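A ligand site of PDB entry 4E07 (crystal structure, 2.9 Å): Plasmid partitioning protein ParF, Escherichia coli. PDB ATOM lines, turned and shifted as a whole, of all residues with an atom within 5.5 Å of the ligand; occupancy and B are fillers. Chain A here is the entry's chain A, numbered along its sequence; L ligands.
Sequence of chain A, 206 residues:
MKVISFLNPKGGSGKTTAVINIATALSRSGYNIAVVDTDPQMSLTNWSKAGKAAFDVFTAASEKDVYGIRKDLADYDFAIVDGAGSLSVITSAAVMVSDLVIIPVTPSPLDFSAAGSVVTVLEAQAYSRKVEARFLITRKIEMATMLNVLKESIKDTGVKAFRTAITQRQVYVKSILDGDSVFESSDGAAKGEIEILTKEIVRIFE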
ATOM      1  N   LYS A  10      26.815 -15.590  23.773  1.00  0.00           N
ATOM      2  CA  LYS A  10      26.154 -15.544  22.482  1.00  0.00           C
ATOM      3  C   LYS A  10      24.665 -15.690  22.655  1.00  0.00           C
ATOM      4  O   LYS A  10      24.150 -16.812  22.707  1.00  0.00           O
ATOM      5  CB  LYS A  10      26.656 -16.658  21.571  1.00  0.00           C
ATOM      6  CG  LYS A  10      26.203 -16.538  20.114  1.00  0.00           C
ATOM      7  CD  LYS A  10      26.749 -15.264  19.461  1.00  0.00           C
ATOM      8  CE  LYS A  10      26.223 -15.103  18.039  1.00  0.00           C
ATOM      9  NZ  LYS A  10      24.733 -15.209  18.006  1.00  0.00           N
ATOM     10  N   GLY A  11      23.948 -14.572  22.755  1.00  0.00           N
ATOM     11  CA  GLY A  11      22.515 -14.670  22.920  1.00  0.00           C
ATOM     12  C   GLY A  11      21.842 -15.494  21.827  1.00  0.00           C
ATOM     13  O   GLY A  11      22.215 -15.398  20.661  1.00  0.00           O
ATOM     14  N   GLY A  12      20.860 -16.303  22.223  1.00  0.00           N
ATOM     15  CA  GLY A  12      20.142 -17.124  21.266  1.00  0.00           C
ATOM     16  C   GLY A  12      20.427 -18.589  21.429  1.00  0.00           C
ATOM     17  O   GLY A  12      19.944 -19.402  20.643  1.00  0.00           O
ATOM     18  N   SER A  13      21.202 -18.934  22.461  1.00  0.00           N
ATOM     19  CA  SER A  13      21.549 -20.327  22.703  1.00  0.00           C
ATOM     20  C   SER A  13      20.569 -21.029  23.654  1.00  0.00           C
ATOM     21  O   SER A  13      20.855 -22.116  24.169  1.00  0.00           O
ATOM     22  CB  SER A  13      22.968 -20.417  23.263  1.00  0.00           C
ATOM     23  OG  SER A  13      23.147 -19.477  24.295  1.00  0.00           O
ATOM     24  N   GLY A  14      19.416 -20.403  23.876  1.00  0.00           N
ATOM     25  CA  GLY A  14      18.391 -20.983  24.718  1.00  0.00           C
ATOM     26  C   GLY A  14      18.574 -21.000  26.235  1.00  0.00           C
ATOM     27  O   GLY A  14      18.118 -21.927  26.909  1.00  0.00           O
ATOM     28  N   LYS A  15      19.242 -19.986  26.771  1.00  0.00           N
ATOM     29  CA  LYS A  15      19.473 -19.922  28.213  1.00  0.00           C
ATOM     30  C   LYS A  15      18.162 -19.798  28.984  1.00  0.00           C
ATOM     31  O   LYS A  15      17.808 -20.714  29.728  1.00  0.00           O
ATOM     32  CB  LYS A  15      20.403 -18.757  28.562  1.00  0.00           C
ATOM     33  CG  LYS A  15      21.873 -19.029  28.176  1.00  0.00           C
ATOM     34  CD  LYS A  15      22.851 -18.027  28.776  1.00  0.00           C
ATOM     35  CE  LYS A  15      22.648 -16.634  28.210  1.00  0.00           C
ATOM     36  NZ  LYS A  15      22.204 -16.662  26.775  1.00  0.00           N
ATOM     37  N   THR A  16      17.455 -18.673  28.803  1.00  0.00           N
ATOM     38  CA  THR A  16      16.192 -18.420  29.471  1.00  0.00           C
ATOM     39  C   THR A  16      15.267 -19.639  29.405  1.00  0.00           C
ATOM     40  O   THR A  16      14.965 -20.272  30.417  1.00  0.00           O
ATOM     41  CB  THR A  16      15.438 -17.231  28.820  1.00  0.00           C
ATOM     42  OG1 THR A  16      16.021 -16.005  29.256  1.00  0.00           O
ATOM     43  CG2 THR A  16      13.957 -17.251  29.190  1.00  0.00           C
ATOM     44  N   THR A  17      14.839 -19.965  28.200  1.00  0.00           N
ATOM     45  CA  THR A  17      13.933 -21.083  27.984  1.00  0.00           C
ATOM     46  C   THR A  17      14.326 -22.364  28.718  1.00  0.00           C
ATOM     47  O   THR A  17      13.488 -22.992  29.349  1.00  0.00           O
ATOM     48  CB  THR A  17      13.796 -21.364  26.476  1.00  0.00           C
ATOM     49  OG1 THR A  17      13.236 -20.218  25.821  1.00  0.00           O
ATOM     50  CG2 THR A  17      12.951 -22.616  26.225  1.00  0.00           C
ATOM     51  N   ALA A  18      15.588 -22.751  28.625  1.00  0.00           N
ATOM     52  CA  ALA A  18      16.056 -23.959  29.306  1.00  0.00           C
ATOM     53  C   ALA A  18      15.900 -23.763  30.807  1.00  0.00           C
ATOM     54  O   ALA A  18      15.382 -24.653  31.506  1.00  0.00           O
ATOM     55  CB  ALA A  18      17.515 -24.252  28.949  1.00  0.00           C
ATOM     56  N   ASP A  39      20.584 -10.996  33.284  1.00  0.00           N
ATOM     57  CA  ASP A  39      20.539 -10.349  31.963  1.00  0.00           C
ATOM     58  C   ASP A  39      19.878  -8.976  31.999  1.00  0.00           C
ATOM     59  O   ASP A  39      18.745  -8.832  32.435  1.00  0.00           O
ATOM     60  CB  ASP A  39      19.808 -11.244  30.962  1.00  0.00           C
ATOM     61  CG  ASP A  39      19.638 -10.589  29.603  1.00  0.00           C
ATOM     62  OD1 ASP A  39      20.605  -9.963  29.123  1.00  0.00           O
ATOM     63  OD2 ASP A  39      18.549 -10.710  29.004  1.00  0.00           O
ATOM     64  N   SER A  43      14.706 -10.603  30.541  1.00  0.00           N
ATOM     65  CA  SER A  43      13.734 -11.414  29.832  1.00  0.00           C
ATOM     66  C   SER A  43      12.968 -12.352  30.762  1.00  0.00           C
ATOM     67  O   SER A  43      11.729 -12.366  30.764  1.00  0.00           O
ATOM     68  CB  SER A  43      14.428 -12.227  28.730  1.00  0.00           C
ATOM     69  OG  SER A  43      14.746 -11.388  27.638  1.00  0.00           O
ATOM     70  N   LEU A  44      13.703 -13.134  31.554  1.00  0.00           N
ATOM     71  CA  LEU A  44      13.066 -14.082  32.471  1.00  0.00           C
ATOM     72  C   LEU A  44      12.251 -13.347  33.516  1.00  0.00           C
ATOM     73  O   LEU A  44      11.248 -13.865  33.992  1.00  0.00           O
ATOM     74  CB  LEU A  44      14.102 -14.989  33.145  1.00  0.00           C
ATOM     75  CG  LEU A  44      13.584 -16.161  34.006  1.00  0.00           C
ATOM     76  CD1 LEU A  44      14.656 -17.255  34.065  1.00  0.00           C
ATOM     77  CD2 LEU A  44      13.249 -15.686  35.417  1.00  0.00           C
ATOM     78  N   ASP A  82      20.412 -17.462  35.367  1.00  0.00           N
ATOM     79  CA  ASP A  82      20.149 -17.256  33.955  1.00  0.00           C
ATOM     80  C   ASP A  82      21.193 -16.280  33.412  1.00  0.00           C
ATOM     81  O   ASP A  82      21.062 -15.071  33.581  1.00  0.00           O
ATOM     82  CB  ASP A  82      18.747 -16.678  33.748  1.00  0.00           C
ATOM     83  CG  ASP A  82      18.354 -16.553  32.282  1.00  0.00           C
ATOM     84  OD1 ASP A  82      17.205 -16.151  32.021  1.00  0.00           O
ATOM     85  OD2 ASP A  82      19.186 -16.857  31.386  1.00  0.00           O
ATOM     86  N   GLY A  83      22.227 -16.801  32.756  1.00  0.00           N
ATOM     87  CA  GLY A  83      23.283 -15.956  32.220  1.00  0.00           C
ATOM     88  C   GLY A  83      22.826 -14.850  31.297  1.00  0.00           C
ATOM     89  O   GLY A  83      21.739 -14.918  30.692  1.00  0.00           O
ATOM     90  N   ALA A  84      23.660 -13.822  31.183  1.00  0.00           N
ATOM     91  CA  ALA A  84      23.389 -12.677  30.318  1.00  0.00           C
ATOM     92  C   ALA A  84      23.974 -12.939  28.918  1.00  0.00           C
ATOM     93  O   ALA A  84      24.798 -13.838  28.738  1.00  0.00           O
ATOM     94  CB  ALA A  84      24.013 -11.407  30.920  1.00  0.00           C
ATOM     95  N   GLY A  85      23.538 -12.149  27.936  1.00  0.00           N
ATOM     96  CA  GLY A  85      24.014 -12.323  26.579  1.00  0.00           C
ATOM     97  C   GLY A  85      25.260 -11.516  26.234  1.00  0.00           C
ATOM     98  O   GLY A  85      25.352 -10.957  25.137  1.00  0.00           O
ATOM     99  N   THR A 138      20.691 -27.131  22.961  1.00  0.00           N
ATOM    100  CA  THR A 138      19.376 -26.506  22.871  1.00  0.00           C
ATOM    101  C   THR A 138      18.929 -26.274  21.425  1.00  0.00           C
ATOM    102  O   THR A 138      19.739 -26.262  20.509  1.00  0.00           O
ATOM    103  CB  THR A 138      19.346 -25.135  23.588  1.00  0.00           C
ATOM    104  OG1 THR A 138      20.238 -25.153  24.714  1.00  0.00           O
ATOM    105  CG2 THR A 138      17.939 -24.839  24.095  1.00  0.00           C
ATOM    106  N   ARG A 139      17.627 -26.077  21.252  1.00  0.00           N
ATOM    107  CA  ARG A 139      17.065 -25.831  19.924  1.00  0.00           C
ATOM    108  C   ARG A 139      17.578 -26.871  18.964  1.00  0.00           C
ATOM    109  O   ARG A 139      18.386 -26.581  18.088  1.00  0.00           O
ATOM    110  CB  ARG A 139      17.449 -24.444  19.430  1.00  0.00           C
ATOM    111  CG  ARG A 139      16.317 -23.439  19.491  1.00  0.00           C
ATOM    112  CD  ARG A 139      16.863 -22.032  19.359  1.00  0.00           C
ATOM    113  NE  ARG A 139      15.831 -21.112  18.885  1.00  0.00           N
ATOM    114  CZ  ARG A 139      15.199 -21.231  17.712  1.00  0.00           C
ATOM    115  NH1 ARG A 139      15.483 -22.246  16.911  1.00  0.00           N
ATOM    116  NH2 ARG A 139      14.294 -20.331  17.339  1.00  0.00           N
ATOM    117  N   ILE A 166      17.249 -30.670  24.063  1.00  0.00           N
ATOM    118  CA  ILE A 166      15.935 -30.047  23.908  1.00  0.00           C
ATOM    119  C   ILE A 166      15.691 -29.732  22.433  1.00  0.00           C
ATOM    120  O   ILE A 166      16.365 -28.890  21.822  1.00  0.00           O
ATOM    121  CB  ILE A 166      15.801 -28.727  24.748  1.00  0.00           C
ATOM    122  CG1 ILE A 166      16.281 -28.934  26.190  1.00  0.00           C
ATOM    123  CG2 ILE A 166      14.356 -28.314  24.820  1.00  0.00           C
ATOM    124  CD1 ILE A 166      17.780 -28.835  26.336  1.00  0.00           C
ATOM    125  N   THR A 167      14.705 -30.411  21.861  1.00  0.00           N
ATOM    126  CA  THR A 167      14.358 -30.233  20.461  1.00  0.00           C
ATOM    127  C   THR A 167      13.702 -28.865  20.238  1.00  0.00           C
ATOM    128  O   THR A 167      13.331 -28.166  21.177  1.00  0.00           O
ATOM    129  CB  THR A 167      13.377 -31.354  20.014  1.00  0.00           C
ATOM    130  OG1 THR A 167      13.697 -32.565  20.704  1.00  0.00           O
ATOM    131  CG2 THR A 167      13.505 -31.603  18.501  1.00  0.00           C
ATOM    132  N   GLN A 168      13.567 -28.467  18.971  1.00  0.00           N
ATOM    133  CA  GLN A 168      12.913 -27.216  18.637  1.00  0.00           C
ATOM    134  C   GLN A 168      11.415 -27.460  18.456  1.00  0.00           C
ATOM    135  O   GLN A 168      10.974 -27.885  17.384  1.00  0.00           O
ATOM    136  CB  GLN A 168      13.477 -26.624  17.352  1.00  0.00           C
ATOM    137  CG  GLN A 168      13.994 -25.193  17.512  1.00  0.00           C
ATOM    138  CD  GLN A 168      13.418 -24.227  16.481  1.00  0.00           C
ATOM    139  OE1 GLN A 168      13.481 -24.464  15.279  1.00  0.00           O
ATOM    140  NE2 GLN A 168      12.845 -23.119  16.965  1.00  0.00           N
ATOM    141  N   ARG A 169      10.639 -27.197  19.499  1.00  0.00           N
ATOM    142  CA  ARG A 169       9.193 -27.377  19.456  1.00  0.00           C
ATOM    143  C   ARG A 169       8.496 -26.023  19.569  1.00  0.00           C
ATOM    144  O   ARG A 169       9.087 -25.047  20.007  1.00  0.00           O
ATOM    145  CB  ARG A 169       8.773 -28.305  20.596  1.00  0.00           C
ATOM    146  CG  ARG A 169       9.622 -29.553  20.664  1.00  0.00           C
ATOM    147  CD  ARG A 169       9.302 -30.354  21.909  1.00  0.00           C
ATOM    148  NE  ARG A 169      10.185 -31.509  22.061  1.00  0.00           N
ATOM    149  CZ  ARG A 169      10.190 -32.559  21.238  1.00  0.00           C
ATOM    150  NH1 ARG A 169       9.371 -32.600  20.199  1.00  0.00           N
ATOM    151  NH2 ARG A 169      11.031 -33.561  21.453  1.00  0.00           N
ATOM    152  N   GLN A 170       7.233 -25.956  19.155  1.00  0.00           N
ATOM    153  CA  GLN A 170       6.487 -24.708  19.207  1.00  0.00           C
ATOM    154  C   GLN A 170       6.036 -24.390  20.630  1.00  0.00           C
ATOM    155  O   GLN A 170       5.887 -23.228  21.007  1.00  0.00           O
ATOM    156  CB  GLN A 170       5.262 -24.785  18.287  1.00  0.00           C
ATOM    157  CG  GLN A 170       5.005 -23.552  17.495  1.00  0.00           C
ATOM    158  CD  GLN A 170       3.970 -23.780  16.439  1.00  0.00           C
ATOM    159  OE1 GLN A 170       4.010 -24.785  15.742  1.00  0.00           O
ATOM    160  NE2 GLN A 170       3.029 -22.854  16.316  1.00  0.00           N
ATOM    161  N   TYR A 172       7.621 -24.588  23.324  1.00  0.00           N
ATOM    162  CA  TYR A 172       8.641 -23.828  24.030  1.00  0.00           C
ATOM    163  C   TYR A 172       8.513 -22.322  23.801  1.00  0.00           C
ATOM    164  O   TYR A 172       8.924 -21.521  24.641  1.00  0.00           O
ATOM    165  CB  TYR A 172      10.017 -24.290  23.593  1.00  0.00           C
ATOM    166  CG  TYR A 172      10.402 -25.612  24.176  1.00  0.00           C
ATOM    167  CD1 TYR A 172      10.774 -26.685  23.345  1.00  0.00           C
ATOM    168  CD2 TYR A 172      10.406 -25.787  25.566  1.00  0.00           C
ATOM    169  CE1 TYR A 172      11.152 -27.916  23.874  1.00  0.00           C
ATOM    170  CE2 TYR A 172      10.779 -27.021  26.125  1.00  0.00           C
ATOM    171  CZ  TYR A 172      11.146 -28.087  25.273  1.00  0.00           C
ATOM    172  OH  TYR A 172      11.478 -29.303  25.811  1.00  0.00           O
ATOM    173  N   VAL A 173       7.962 -21.926  22.664  1.00  0.00           N
ATOM    174  CA  VAL A 173       7.805 -20.520  22.371  1.00  0.00           C
ATOM    175  C   VAL A 173       6.444 -20.027  22.835  1.00  0.00           C
ATOM    176  O   VAL A 173       6.315 -18.917  23.378  1.00  0.00           O
ATOM    177  CB  VAL A 173       7.958 -20.226  20.875  1.00  0.00           C
ATOM    178  CG1 VAL A 173       7.863 -18.737  20.611  1.00  0.00           C
ATOM    179  CG2 VAL A 173       9.280 -20.769  20.394  1.00  0.00           C
ATOM    180  N   ILE A 176       6.130 -19.357  26.736  1.00  0.00           N
ATOM    181  CA  ILE A 176       6.588 -18.038  27.181  1.00  0.00           C
ATOM    182  C   ILE A 176       5.523 -16.954  26.933  1.00  0.00           C
ATOM    183  O   ILE A 176       5.294 -16.083  27.784  1.00  0.00           O
ATOM    184  CB  ILE A 176       7.903 -17.613  26.445  1.00  0.00           C
ATOM    185  CG1 ILE A 176       8.983 -18.672  26.634  1.00  0.00           C
ATOM    186  CG2 ILE A 176       8.358 -16.232  26.942  1.00  0.00           C
ATOM    187  CD1 ILE A 176       9.365 -18.909  28.061  1.00  0.00           C
HETATM  188  P1  LIG L   1      18.377 -15.034  27.853  1.00  0.00           P
HETATM  189  O1  LIG L   1      18.645 -15.915  29.008  1.00  0.00           O
HETATM  190  O2  LIG L   1      17.263 -14.094  28.037  1.00  0.00           O
HETATM  191  O3  LIG L   1      19.630 -14.296  27.475  1.00  0.00           O
HETATM  192  P2  LIG L   1      19.021 -16.468  25.438  1.00  0.00           P
HETATM  193  O4  LIG L   1      19.117 -15.566  24.276  1.00  0.00           O
HETATM  194  O5  LIG L   1      19.641 -17.727  25.735  1.00  0.00           O
HETATM  195  C1  LIG L   1      17.921 -15.951  26.578  1.00  0.00           C
HETATM  196  P3  LIG L   1      16.333 -17.631  24.636  1.00  0.00           P
HETATM  197  O6  LIG L   1      16.225 -18.735  25.614  1.00  0.00           O
HETATM  198  O7  LIG L   1      15.470 -16.417  24.820  1.00  0.00           O
HETATM  199  O8  LIG L   1      17.906 -17.182  24.548  1.00  0.00           O
HETATM  200  O9  LIG L   1      16.095 -18.278  23.202  1.00  0.00           O
HETATM  201  C2  LIG L   1      16.248 -17.516  21.968  1.00  0.00           C
HETATM  202  C3  LIG L   1      15.056 -17.694  21.046  1.00  0.00           C
HETATM  203  O10 LIG L   1      14.909 -19.096  20.793  1.00  0.00           O
HETATM  204  C4  LIG L   1      13.742 -17.250  21.572  1.00  0.00           C
HETATM  205  O11 LIG L   1      13.106 -16.544  20.490  1.00  0.00           O
HETATM  206  C5  LIG L   1      13.058 -18.527  22.011  1.00  0.00           C
HETATM  207  O12 LIG L   1      11.635 -18.479  21.987  1.00  0.00           O
HETATM  208  C6  LIG L   1      13.592 -19.585  21.083  1.00  0.00           C
HETATM  209  N1  LIG L   1      13.783 -20.938  21.652  1.00  0.00           N
HETATM  210  C7  LIG L   1      14.622 -21.357  22.663  1.00  0.00           C
HETATM  211  N2  LIG L   1      14.571 -22.633  22.923  1.00  0.00           N
HETATM  212  C8  LIG L   1      13.641 -23.085  22.006  1.00  0.00           C
HETATM  213  C9  LIG L   1      13.098 -24.394  21.726  1.00  0.00           C
HETATM  214  N3  LIG L   1      13.511 -25.471  22.407  1.00  0.00           N
HETATM  215  N4  LIG L   1      12.152 -24.546  20.724  1.00  0.00           N
HETATM  216  C10 LIG L   1      11.733 -23.456  20.030  1.00  0.00           C
HETATM  217  N5  LIG L   1      12.171 -22.170  20.197  1.00  0.00           N
HETATM  218  C11 LIG L   1      13.135 -22.059  21.224  1.00  0.00           C
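Residues that only touch the ligand: Tyr 172, Val 173, Ser 43, Gly 83, Gly 11, Asp 39, Ser 13 and Ile 166.
Hydrophobic or aromatic side chains within 4 Å of the ligand: Ile 166, Tyr 172 and Val 173.
Within 4 Å of the ligand: Gly 11, Gly 12, Ser 13, Gly 14, Lys 15, Thr 16, Thr 17, Asp 39, Ser 43, Asp 82, Gly 83, Arg 139, Ile 166, Thr 167, Gln 168, Arg 169, Tyr 172 and Val 173.
The backbone NH of Lys 15 lies within hydrogen-bond range of an oxygen (O5) of the ligand (2.5 Å).
N of Gly 12 lies within hydrogen-bond range of O4 of the ligand.
An oxygen (O6) of the ligand lies within hydrogen-bond range of the side-chain hydroxyl (OG1) of Thr 17 (3.3 Å).
The backbone carbonyl oxygen (O) of Thr 167 lies within hydrogen-bond range of a nitrogen (N3) of the ligand, at 3.0 Å.
The backbone NH (N) of Arg 169 lies within hydrogen-bond range of a nitrogen (N4) of the ligand (3.3 Å).
An oxygen (O6) of the ligand is in hydrogen-bond range of the backbone NH of Thr 17 (3.2 Å).
The side-chain carboxylate (OD2) of Asp 82 lies close to an oxygen (O1) of the ligand.
N5 of the ligand lies close to NE2 of Gln 168, 3.4 Å away.
The side-chain amino group (NZ) of Lys 15 is in salt-bridge range of an oxygen (O5) of the ligand, at 3.0 Å.
The backbone NH of Gly 14 lies within hydrogen-bond range of an oxygen (O5) of the ligand, 3.3 Å away.
The side-chain hydroxyl (OG1) of Thr 16 is in hydrogen-bond range of an oxygen (O2) of the ligand (2.6 Å).
The backbone NH (N) of Thr 16 sits at hydrogen-bond distance from an oxygen (O1) of the ligand (3.0 Å).
An oxygen (O10) of the ligand is in hydrogen-bond range of the guanidinium group (NE) of Arg 139 (2.9 Å).
The guanidinium group (NH1) of Arg 139 lies close to the side-chain amide nitrogen (NE2) of Gln 168, 2.8 Å away.
The side-chain carboxylate (OD1) of Asp 82 sits at hydrogen-bond distance from the side-chain hydroxyl (OG1) of Thr 16.
The side-chain hydroxyl (OG) of Ser 13 lies within hydrogen-bond range of the backbone carbonyl oxygen (O) of Lys 10 (3.3 Å).
N of Arg 139 sits at hydrogen-bond distance from O of Ile 166.
The backbone carbonyl oxygen (O) of Ser 13 is in hydrogen-bond range of the side-chain hydroxyl (OG1) of Thr 138, 3.1 Å away.
The side-chain hydroxyl (OG1) of Thr 167 is in hydrogen-bond range of the guanidinium group (NH2) of Arg 169 (2.9 Å).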
